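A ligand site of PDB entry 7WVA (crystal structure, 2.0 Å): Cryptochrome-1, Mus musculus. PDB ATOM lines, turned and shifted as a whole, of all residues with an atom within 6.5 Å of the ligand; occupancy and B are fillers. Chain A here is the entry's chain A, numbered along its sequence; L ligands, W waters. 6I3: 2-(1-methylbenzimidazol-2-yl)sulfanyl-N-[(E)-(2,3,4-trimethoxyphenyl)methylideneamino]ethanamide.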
ATOM      1  N   GLY A 290      11.152 -32.492  19.682  1.00  0.00           N
ATOM      2  CA  GLY A 290      10.499 -31.565  18.762  1.00  0.00           C
ATOM      3  C   GLY A 290      10.014 -32.224  17.476  1.00  0.00           C
ATOM      4  O   GLY A 290       8.891 -31.975  17.027  1.00  0.00           O
ATOM      5  N   GLN A 291      10.864 -33.046  16.862  1.00  0.00           N
ATOM      6  CA  GLN A 291      10.463 -33.737  15.640  1.00  0.00           C
ATOM      7  C   GLN A 291       9.172 -34.510  15.850  1.00  0.00           C
ATOM      8  O   GLN A 291       8.234 -34.425  15.044  1.00  0.00           O
ATOM      9  CB  GLN A 291      11.590 -34.675  15.174  1.00  0.00           C
ATOM     10  CG  GLN A 291      11.230 -35.518  13.948  1.00  0.00           C
ATOM     11  CD  GLN A 291      12.373 -36.440  13.491  1.00  0.00           C
ATOM     12  OE1 GLN A 291      13.365 -36.611  14.181  1.00  0.00           O
ATOM     13  NE2 GLN A 291      12.210 -37.033  12.302  1.00  0.00           N
ATOM     14  N   LEU A 292       9.088 -35.272  16.942  1.00  0.00           N
ATOM     15  CA  LEU A 292       7.907 -36.093  17.208  1.00  0.00           C
ATOM     16  C   LEU A 292       6.725 -35.276  17.698  1.00  0.00           C
ATOM     17  O   LEU A 292       5.563 -35.664  17.481  1.00  0.00           O
ATOM     18  CB  LEU A 292       8.262 -37.169  18.221  1.00  0.00           C
ATOM     19  CG  LEU A 292       9.334 -38.172  17.815  1.00  0.00           C
ATOM     20  CD1 LEU A 292       9.708 -39.019  19.025  1.00  0.00           C
ATOM     21  CD2 LEU A 292       8.813 -39.046  16.677  1.00  0.00           C
ATOM     22  N   TRP A 294       5.969 -31.963  17.029  1.00  0.00           N
ATOM     23  CA  TRP A 294       5.358 -31.243  15.918  1.00  0.00           C
ATOM     24  C   TRP A 294       4.486 -32.176  15.098  1.00  0.00           C
ATOM     25  O   TRP A 294       3.349 -31.821  14.741  1.00  0.00           O
ATOM     26  CB  TRP A 294       6.436 -30.615  15.028  1.00  0.00           C
ATOM     27  CG  TRP A 294       6.799 -29.235  15.428  1.00  0.00           C
ATOM     28  CD1 TRP A 294       7.933 -28.837  16.095  1.00  0.00           C
ATOM     29  CD2 TRP A 294       6.023 -28.061  15.215  1.00  0.00           C
ATOM     30  NE1 TRP A 294       7.906 -27.475  16.294  1.00  0.00           N
ATOM     31  CE2 TRP A 294       6.736 -26.975  15.755  1.00  0.00           C
ATOM     32  CE3 TRP A 294       4.785 -27.806  14.603  1.00  0.00           C
ATOM     33  CZ2 TRP A 294       6.266 -25.663  15.705  1.00  0.00           C
ATOM     34  CZ3 TRP A 294       4.323 -26.498  14.553  1.00  0.00           C
ATOM     35  CH2 TRP A 294       5.065 -25.453  15.103  1.00  0.00           C
ATOM     36  N   ARG A 295       4.998 -33.373  14.809  1.00  0.00           N
ATOM     37  CA  ARG A 295       4.234 -34.394  14.110  1.00  0.00           C
ATOM     38  C   ARG A 295       2.942 -34.700  14.841  1.00  0.00           C
ATOM     39  O   ARG A 295       1.861 -34.716  14.243  1.00  0.00           O
ATOM     40  CB  ARG A 295       5.125 -35.632  13.977  1.00  0.00           C
ATOM     41  CG  ARG A 295       4.500 -36.883  13.454  1.00  0.00           C
ATOM     42  CD  ARG A 295       5.590 -38.012  13.531  1.00  0.00           C
ATOM     43  NE  ARG A 295       5.162 -39.249  12.898  1.00  0.00           N
ATOM     44  CZ  ARG A 295       4.577 -40.247  13.547  1.00  0.00           C
ATOM     45  NH1 ARG A 295       4.334 -40.186  14.851  1.00  0.00           N
ATOM     46  NH2 ARG A 295       4.214 -41.333  12.867  1.00  0.00           N
ATOM     47  N   PHE A 298       0.294 -31.795  14.567  1.00  0.00           N
ATOM     48  CA  PHE A 298      -0.499 -31.721  13.345  1.00  0.00           C
ATOM     49  C   PHE A 298      -1.501 -32.870  13.246  1.00  0.00           C
ATOM     50  O   PHE A 298      -2.619 -32.667  12.790  1.00  0.00           O
ATOM     51  CB  PHE A 298       0.411 -31.672  12.117  1.00  0.00           C
ATOM     52  CG  PHE A 298       1.022 -30.312  11.869  1.00  0.00           C
ATOM     53  CD1 PHE A 298       0.310 -29.167  12.134  1.00  0.00           C
ATOM     54  CD2 PHE A 298       2.311 -30.189  11.391  1.00  0.00           C
ATOM     55  CE1 PHE A 298       0.861 -27.911  11.911  1.00  0.00           C
ATOM     56  CE2 PHE A 298       2.869 -28.942  11.160  1.00  0.00           C
ATOM     57  CZ  PHE A 298       2.155 -27.803  11.417  1.00  0.00           C
ATOM     58  N   HIS A 357      14.105 -29.423   5.734  1.00  0.00           N
ATOM     59  CA  HIS A 357      12.934 -28.606   6.096  1.00  0.00           C
ATOM     60  C   HIS A 357      13.120 -27.125   5.771  1.00  0.00           C
ATOM     61  O   HIS A 357      12.167 -26.466   5.365  1.00  0.00           O
ATOM     62  CB  HIS A 357      12.567 -28.800   7.573  1.00  0.00           C
ATOM     63  CG  HIS A 357      13.602 -28.354   8.556  1.00  0.00           C
ATOM     64  ND1 HIS A 357      14.534 -29.217   9.098  1.00  0.00           N
ATOM     65  CD2 HIS A 357      13.791 -27.159   9.179  1.00  0.00           C
ATOM     66  CE1 HIS A 357      15.291 -28.569   9.960  1.00  0.00           C
ATOM     67  NE2 HIS A 357      14.863 -27.316  10.039  1.00  0.00           N
ATOM     68  N   LEU A 358      14.332 -26.570   5.921  1.00  0.00           N
ATOM     69  CA  LEU A 358      14.493 -25.157   5.550  1.00  0.00           C
ATOM     70  C   LEU A 358      14.463 -24.972   4.031  1.00  0.00           C
ATOM     71  O   LEU A 358      14.102 -23.887   3.562  1.00  0.00           O
ATOM     72  CB  LEU A 358      15.780 -24.575   6.136  1.00  0.00           C
ATOM     73  CG  LEU A 358      15.745 -24.294   7.645  1.00  0.00           C
ATOM     74  CD1 LEU A 358      17.104 -23.775   8.132  1.00  0.00           C
ATOM     75  CD2 LEU A 358      14.608 -23.322   8.015  1.00  0.00           C
ATOM     76  N   ARG A 360      12.327 -26.752   2.318  1.00  0.00           N
ATOM     77  CA  ARG A 360      10.873 -26.713   2.188  1.00  0.00           C
ATOM     78  C   ARG A 360      10.348 -25.315   2.440  1.00  0.00           C
ATOM     79  O   ARG A 360       9.500 -24.837   1.685  1.00  0.00           O
ATOM     80  CB  ARG A 360      10.230 -27.723   3.148  1.00  0.00           C
ATOM     81  CG  ARG A 360      10.567 -29.168   2.852  1.00  0.00           C
ATOM     82  CD  ARG A 360      10.111 -30.135   3.984  1.00  0.00           C
ATOM     83  NE  ARG A 360      10.913 -31.354   3.984  1.00  0.00           N
ATOM     84  CZ  ARG A 360      10.512 -32.518   4.491  1.00  0.00           C
ATOM     85  NH1 ARG A 360       9.294 -32.652   5.021  1.00  0.00           N
ATOM     86  NH2 ARG A 360      11.329 -33.580   4.429  1.00  0.00           N
ATOM     87  N   HIS A 361      10.807 -24.669   3.530  1.00  0.00           N
ATOM     88  CA  HIS A 361      10.382 -23.292   3.833  1.00  0.00           C
ATOM     89  C   HIS A 361      10.628 -22.377   2.641  1.00  0.00           C
ATOM     90  O   HIS A 361       9.783 -21.539   2.308  1.00  0.00           O
ATOM     91  CB  HIS A 361      11.138 -22.734   5.033  1.00  0.00           C
ATOM     92  CG  HIS A 361      10.755 -23.324   6.355  1.00  0.00           C
ATOM     93  ND1 HIS A 361      10.805 -22.604   7.535  1.00  0.00           N
ATOM     94  CD2 HIS A 361      10.316 -24.563   6.700  1.00  0.00           C
ATOM     95  CE1 HIS A 361      10.423 -23.366   8.541  1.00  0.00           C
ATOM     96  NE2 HIS A 361      10.125 -24.568   8.062  1.00  0.00           N
ATOM     97  N   VAL A 363      10.992 -23.064  -0.750  1.00  0.00           N
ATOM     98  CA  VAL A 363      10.135 -23.254  -1.933  1.00  0.00           C
ATOM     99  C   VAL A 363       8.667 -22.992  -1.604  1.00  0.00           C
ATOM    100  O   VAL A 363       7.899 -22.556  -2.475  1.00  0.00           O
ATOM    101  CB  VAL A 363      10.351 -24.652  -2.542  1.00  0.00           C
ATOM    102  CG1 VAL A 363      11.826 -24.807  -3.035  1.00  0.00           C
ATOM    103  CG2 VAL A 363       9.996 -25.779  -1.549  1.00  0.00           C
ATOM    104  N   ALA A 364       8.242 -23.228  -0.357  1.00  0.00           N
ATOM    105  CA  ALA A 364       6.867 -22.913   0.048  1.00  0.00           C
ATOM    106  C   ALA A 364       6.647 -21.408   0.122  1.00  0.00           C
ATOM    107  O   ALA A 364       5.605 -20.908  -0.325  1.00  0.00           O
ATOM    108  CB  ALA A 364       6.553 -23.548   1.396  1.00  0.00           C
ATOM    109  N   PHE A 383       3.818 -31.541  -3.018  1.00  0.00           N
ATOM    110  CA  PHE A 383       4.551 -32.278  -1.990  1.00  0.00           C
ATOM    111  C   PHE A 383       3.936 -33.651  -1.744  1.00  0.00           C
ATOM    112  O   PHE A 383       4.655 -34.630  -1.478  1.00  0.00           O
ATOM    113  CB  PHE A 383       4.605 -31.488  -0.686  1.00  0.00           C
ATOM    114  CG  PHE A 383       5.718 -30.473  -0.622  1.00  0.00           C
ATOM    115  CD1 PHE A 383       6.247 -29.922  -1.792  1.00  0.00           C
ATOM    116  CD2 PHE A 383       6.238 -30.070   0.609  1.00  0.00           C
ATOM    117  CE1 PHE A 383       7.260 -28.977  -1.728  1.00  0.00           C
ATOM    118  CE2 PHE A 383       7.265 -29.145   0.672  1.00  0.00           C
ATOM    119  CZ  PHE A 383       7.773 -28.594  -0.493  1.00  0.00           C
ATOM    120  N   LEU A 387       6.918 -36.046  -1.912  1.00  0.00           N
ATOM    121  CA  LEU A 387       7.625 -36.065  -0.644  1.00  0.00           C
ATOM    122  C   LEU A 387       7.335 -37.364   0.079  1.00  0.00           C
ATOM    123  O   LEU A 387       6.171 -37.757   0.240  1.00  0.00           O
ATOM    124  CB  LEU A 387       7.212 -34.858   0.187  1.00  0.00           C
ATOM    125  CG  LEU A 387       7.991 -34.444   1.432  1.00  0.00           C
ATOM    126  CD1 LEU A 387       9.472 -34.262   1.151  1.00  0.00           C
ATOM    127  CD2 LEU A 387       7.342 -33.129   1.974  1.00  0.00           C
ATOM    128  N   ASP A 389       7.964 -38.160   3.309  1.00  0.00           N
ATOM    129  CA  ASP A 389       7.698 -38.134   4.743  1.00  0.00           C
ATOM    130  C   ASP A 389       6.483 -37.291   5.149  1.00  0.00           C
ATOM    131  O   ASP A 389       6.283 -37.054   6.344  1.00  0.00           O
ATOM    132  CB  ASP A 389       8.940 -37.644   5.492  1.00  0.00           C
ATOM    133  CG  ASP A 389       9.289 -36.183   5.202  1.00  0.00           C
ATOM    134  OD1 ASP A 389       8.499 -35.487   4.530  1.00  0.00           O
ATOM    135  OD2 ASP A 389      10.356 -35.707   5.669  1.00  0.00           O
ATOM    136  N   ALA A 390       5.693 -36.798   4.206  1.00  0.00           N
ATOM    137  CA  ALA A 390       4.604 -35.872   4.559  1.00  0.00           C
ATOM    138  C   ALA A 390       3.263 -36.486   4.209  1.00  0.00           C
ATOM    139  O   ALA A 390       2.844 -36.467   3.055  1.00  0.00           O
ATOM    140  CB  ALA A 390       4.761 -34.529   3.864  1.00  0.00           C
ATOM    141  N   ILE A 394       0.344 -33.869   8.197  1.00  0.00           N
ATOM    142  CA  ILE A 394       1.564 -33.089   8.350  1.00  0.00           C
ATOM    143  C   ILE A 394       1.693 -32.114   7.196  1.00  0.00           C
ATOM    144  O   ILE A 394       2.014 -30.937   7.387  1.00  0.00           O
ATOM    145  CB  ILE A 394       2.804 -34.011   8.455  1.00  0.00           C
ATOM    146  CG1 ILE A 394       2.969 -34.586   9.864  1.00  0.00           C
ATOM    147  CG2 ILE A 394       4.065 -33.260   8.105  1.00  0.00           C
ATOM    148  CD1 ILE A 394       1.846 -35.482  10.329  1.00  0.00           C
ATOM    149  N   ASN A 395       1.455 -32.592   5.983  1.00  0.00           N
ATOM    150  CA  ASN A 395       1.608 -31.785   4.779  1.00  0.00           C
ATOM    151  C   ASN A 395       0.660 -30.588   4.818  1.00  0.00           C
ATOM    152  O   ASN A 395       1.090 -29.433   4.647  1.00  0.00           O
ATOM    153  CB  ASN A 395       1.328 -32.672   3.551  1.00  0.00           C
ATOM    154  CG  ASN A 395       1.926 -32.136   2.274  1.00  0.00           C
ATOM    155  OD1 ASN A 395       2.843 -31.310   2.296  1.00  0.00           O
ATOM    156  ND2 ASN A 395       1.415 -32.603   1.135  1.00  0.00           N
ATOM    157  N   ALA A 396      -0.627 -30.823   5.087  1.00  0.00           N
ATOM    158  CA  ALA A 396      -1.586 -29.714   5.178  1.00  0.00           C
ATOM    159  C   ALA A 396      -1.185 -28.728   6.269  1.00  0.00           C
ATOM    160  O   ALA A 396      -1.098 -27.521   6.024  1.00  0.00           O
ATOM    161  CB  ALA A 396      -2.989 -30.267   5.412  1.00  0.00           C
ATOM    162  N   SER A 398       1.704 -28.129   7.706  1.00  0.00           N
ATOM    163  CA  SER A 398       2.938 -27.424   7.420  1.00  0.00           C
ATOM    164  C   SER A 398       2.718 -26.358   6.355  1.00  0.00           C
ATOM    165  O   SER A 398       3.348 -25.295   6.410  1.00  0.00           O
ATOM    166  CB  SER A 398       4.014 -28.415   6.930  1.00  0.00           C
ATOM    167  OG  SER A 398       4.224 -29.451   7.877  1.00  0.00           O
ATOM    168  N   TRP A 399       1.846 -26.620   5.376  1.00  0.00           N
ATOM    169  CA  TRP A 399       1.622 -25.650   4.305  1.00  0.00           C
ATOM    170  C   TRP A 399       0.791 -24.482   4.796  1.00  0.00           C
ATOM    171  O   TRP A 399       1.022 -23.346   4.376  1.00  0.00           O
ATOM    172  CB  TRP A 399       0.970 -26.330   3.101  1.00  0.00           C
ATOM    173  CG  TRP A 399       1.985 -26.902   2.157  1.00  0.00           C
ATOM    174  CD1 TRP A 399       2.432 -28.192   2.124  1.00  0.00           C
ATOM    175  CD2 TRP A 399       2.702 -26.185   1.147  1.00  0.00           C
ATOM    176  NE1 TRP A 399       3.392 -28.327   1.138  1.00  0.00           N
ATOM    177  CE2 TRP A 399       3.581 -27.101   0.529  1.00  0.00           C
ATOM    178  CE3 TRP A 399       2.693 -24.860   0.707  1.00  0.00           C
ATOM    179  CZ2 TRP A 399       4.426 -26.736  -0.516  1.00  0.00           C
ATOM    180  CZ3 TRP A 399       3.539 -24.490  -0.330  1.00  0.00           C
ATOM    181  CH2 TRP A 399       4.389 -25.429  -0.925  1.00  0.00           C
ATOM    182  N   TRP A 401       0.887 -23.463   7.912  1.00  0.00           N
ATOM    183  CA  TRP A 401       1.818 -22.776   8.802  1.00  0.00           C
ATOM    184  C   TRP A 401       2.736 -21.856   8.022  1.00  0.00           C
ATOM    185  O   TRP A 401       2.851 -20.662   8.341  1.00  0.00           O
ATOM    186  CB  TRP A 401       2.621 -23.820   9.591  1.00  0.00           C
ATOM    187  CG  TRP A 401       3.688 -23.255  10.507  1.00  0.00           C
ATOM    188  CD1 TRP A 401       3.505 -22.357  11.521  1.00  0.00           C
ATOM    189  CD2 TRP A 401       5.087 -23.564  10.504  1.00  0.00           C
ATOM    190  NE1 TRP A 401       4.699 -22.087  12.138  1.00  0.00           N
ATOM    191  CE2 TRP A 401       5.686 -22.825  11.542  1.00  0.00           C
ATOM    192  CE3 TRP A 401       5.873 -24.416   9.740  1.00  0.00           C
ATOM    193  CZ2 TRP A 401       7.055 -22.893  11.814  1.00  0.00           C
ATOM    194  CZ3 TRP A 401       7.245 -24.476  10.006  1.00  0.00           C
ATOM    195  CH2 TRP A 401       7.818 -23.719  11.038  1.00  0.00           C
ATOM    196  N   LEU A 402       3.384 -22.384   6.967  1.00  0.00           N
ATOM    197  CA  LEU A 402       4.341 -21.621   6.175  1.00  0.00           C
ATOM    198  C   LEU A 402       3.708 -20.464   5.438  1.00  0.00           C
ATOM    199  O   LEU A 402       4.334 -19.412   5.277  1.00  0.00           O
ATOM    200  CB  LEU A 402       5.042 -22.530   5.149  1.00  0.00           C
ATOM    201  CG  LEU A 402       6.538 -22.808   5.348  1.00  0.00           C
ATOM    202  CD1 LEU A 402       7.364 -21.526   5.249  1.00  0.00           C
ATOM    203  CD2 LEU A 402       6.757 -23.467   6.690  1.00  0.00           C
HETATM  204  C10 6I3 L   1      11.003 -26.728  10.974  1.00  0.00           C
HETATM  205  C17 6I3 L   1       7.557 -29.745  11.836  1.00  0.00           C
HETATM  206  C20 6I3 L   1       6.804 -32.375  11.290  1.00  0.00           C
HETATM  207  C21 6I3 L   1       7.971 -32.153  11.984  1.00  0.00           C
HETATM  208  C24 6I3 L   1       7.801 -29.531   6.583  1.00  0.00           C
HETATM  209  C26 6I3 L   1       7.149 -31.563   7.688  1.00  0.00           C
HETATM  210  C01 6I3 L   1       5.993 -26.590   3.260  1.00  0.00           C
HETATM  211  C03 6I3 L   1       6.752 -28.048   4.913  1.00  0.00           C
HETATM  212  C04 6I3 L   1       7.153 -26.945   5.684  1.00  0.00           C
HETATM  213  C05 6I3 L   1       7.853 -27.131   6.871  1.00  0.00           C
HETATM  214  C06 6I3 L   1       8.197 -28.411   7.356  1.00  0.00           C
HETATM  215  C07 6I3 L   1       8.946 -28.520   8.614  1.00  0.00           C
HETATM  216  C12 6I3 L   1      11.707 -26.989  12.338  1.00  0.00           C
HETATM  217  C14 6I3 L   1       9.380 -28.946  12.957  1.00  0.00           C
HETATM  218  C16 6I3 L   1       8.381 -30.818  12.266  1.00  0.00           C
HETATM  219  C18 6I3 L   1       6.363 -29.985  11.124  1.00  0.00           C
HETATM  220  C19 6I3 L   1       5.990 -31.276  10.864  1.00  0.00           C
HETATM  221  C23 6I3 L   1       7.742 -27.215  12.049  1.00  0.00           C
HETATM  222  C27 6I3 L   1       7.074 -29.360   5.363  1.00  0.00           C
HETATM  223  C29 6I3 L   1       5.340 -30.764   4.408  1.00  0.00           C
HETATM  224  N08 6I3 L   1       9.848 -27.676   9.052  1.00  0.00           N
HETATM  225  N09 6I3 L   1      10.476 -27.856  10.215  1.00  0.00           N
HETATM  226  N15 6I3 L   1       9.520 -30.290  12.965  1.00  0.00           N
HETATM  227  N22 6I3 L   1       8.192 -28.554  12.273  1.00  0.00           N
HETATM  228  O02 6I3 L   1       6.068 -27.907   3.741  1.00  0.00           O
HETATM  229  O11 6I3 L   1      10.882 -25.623  10.555  1.00  0.00           O
HETATM  230  O25 6I3 L   1       8.125 -30.777   7.000  1.00  0.00           O
HETATM  231  O28 6I3 L   1       6.743 -30.476   4.658  1.00  0.00           O
HETATM  232  S13 6I3 L   1      10.482 -27.671  13.628  1.00  0.00           S
HETATM  233  O   HOH W   1       7.656 -34.946   8.021  1.00  0.00           O
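O11 of the ligand sits at hydrogen-bond distance from NE2 of His 361 (2.8 Å). NH1 of Arg 360 is in hydrogen-bond range of O25 of the ligand, 3.0 Å away. S13 of the ligand sits close to NE1 of Trp 294 (3.7 Å).
The side-chain carboxylate (OD2) of Asp 389 is in salt-bridge range of the guanidinium group (NH2) of Arg 360, at 2.6 Å. OD1 of Asn 395 sits close to NE1 of Trp 399, at 3.2 Å. OG of Ser 398 sits at hydrogen-bond distance from O of Ile 394, 2.7 Å away.
Merely in contact with the ligand: His 357 (3.3 Å), Asn 395 (3.3 Å), Ser 398 (3.4 Å), Trp 401 (3.5 Å), Phe 383 (3.5 Å), Ile 394 (3.5 Å), Ala 364 (3.6 Å), Leu 402 (3.6 Å), Phe 298 (3.6 Å), Trp 399 (3.7 Å), Gln 291 (3.8 Å), Leu 387 (3.8 Å) and Ala 390 (3.8 Å). Hydrophobic or aromatic side chains that line the ligand: Trp 294, Phe 298, His 357, His 361, Ala 364, Phe 383, Leu 387, Ala 390, Ile 394, Trp 399, Trp 401 and Leu 402. Within 4 Å of the ligand: Gln 291, Trp 294, Phe 298, His 357, Arg 360, His 361, Ala 364, Phe 383, Leu 387, Ala 390, Ile 394, Asn 395, Ser 398, Trp 399, Trp 401 and Leu 402. Along chain A the residues within 4 Å of the ligand span positions 291 to 402. The nearest printed residue that does not touch the ligand is Arg 295 (4.1 Å).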
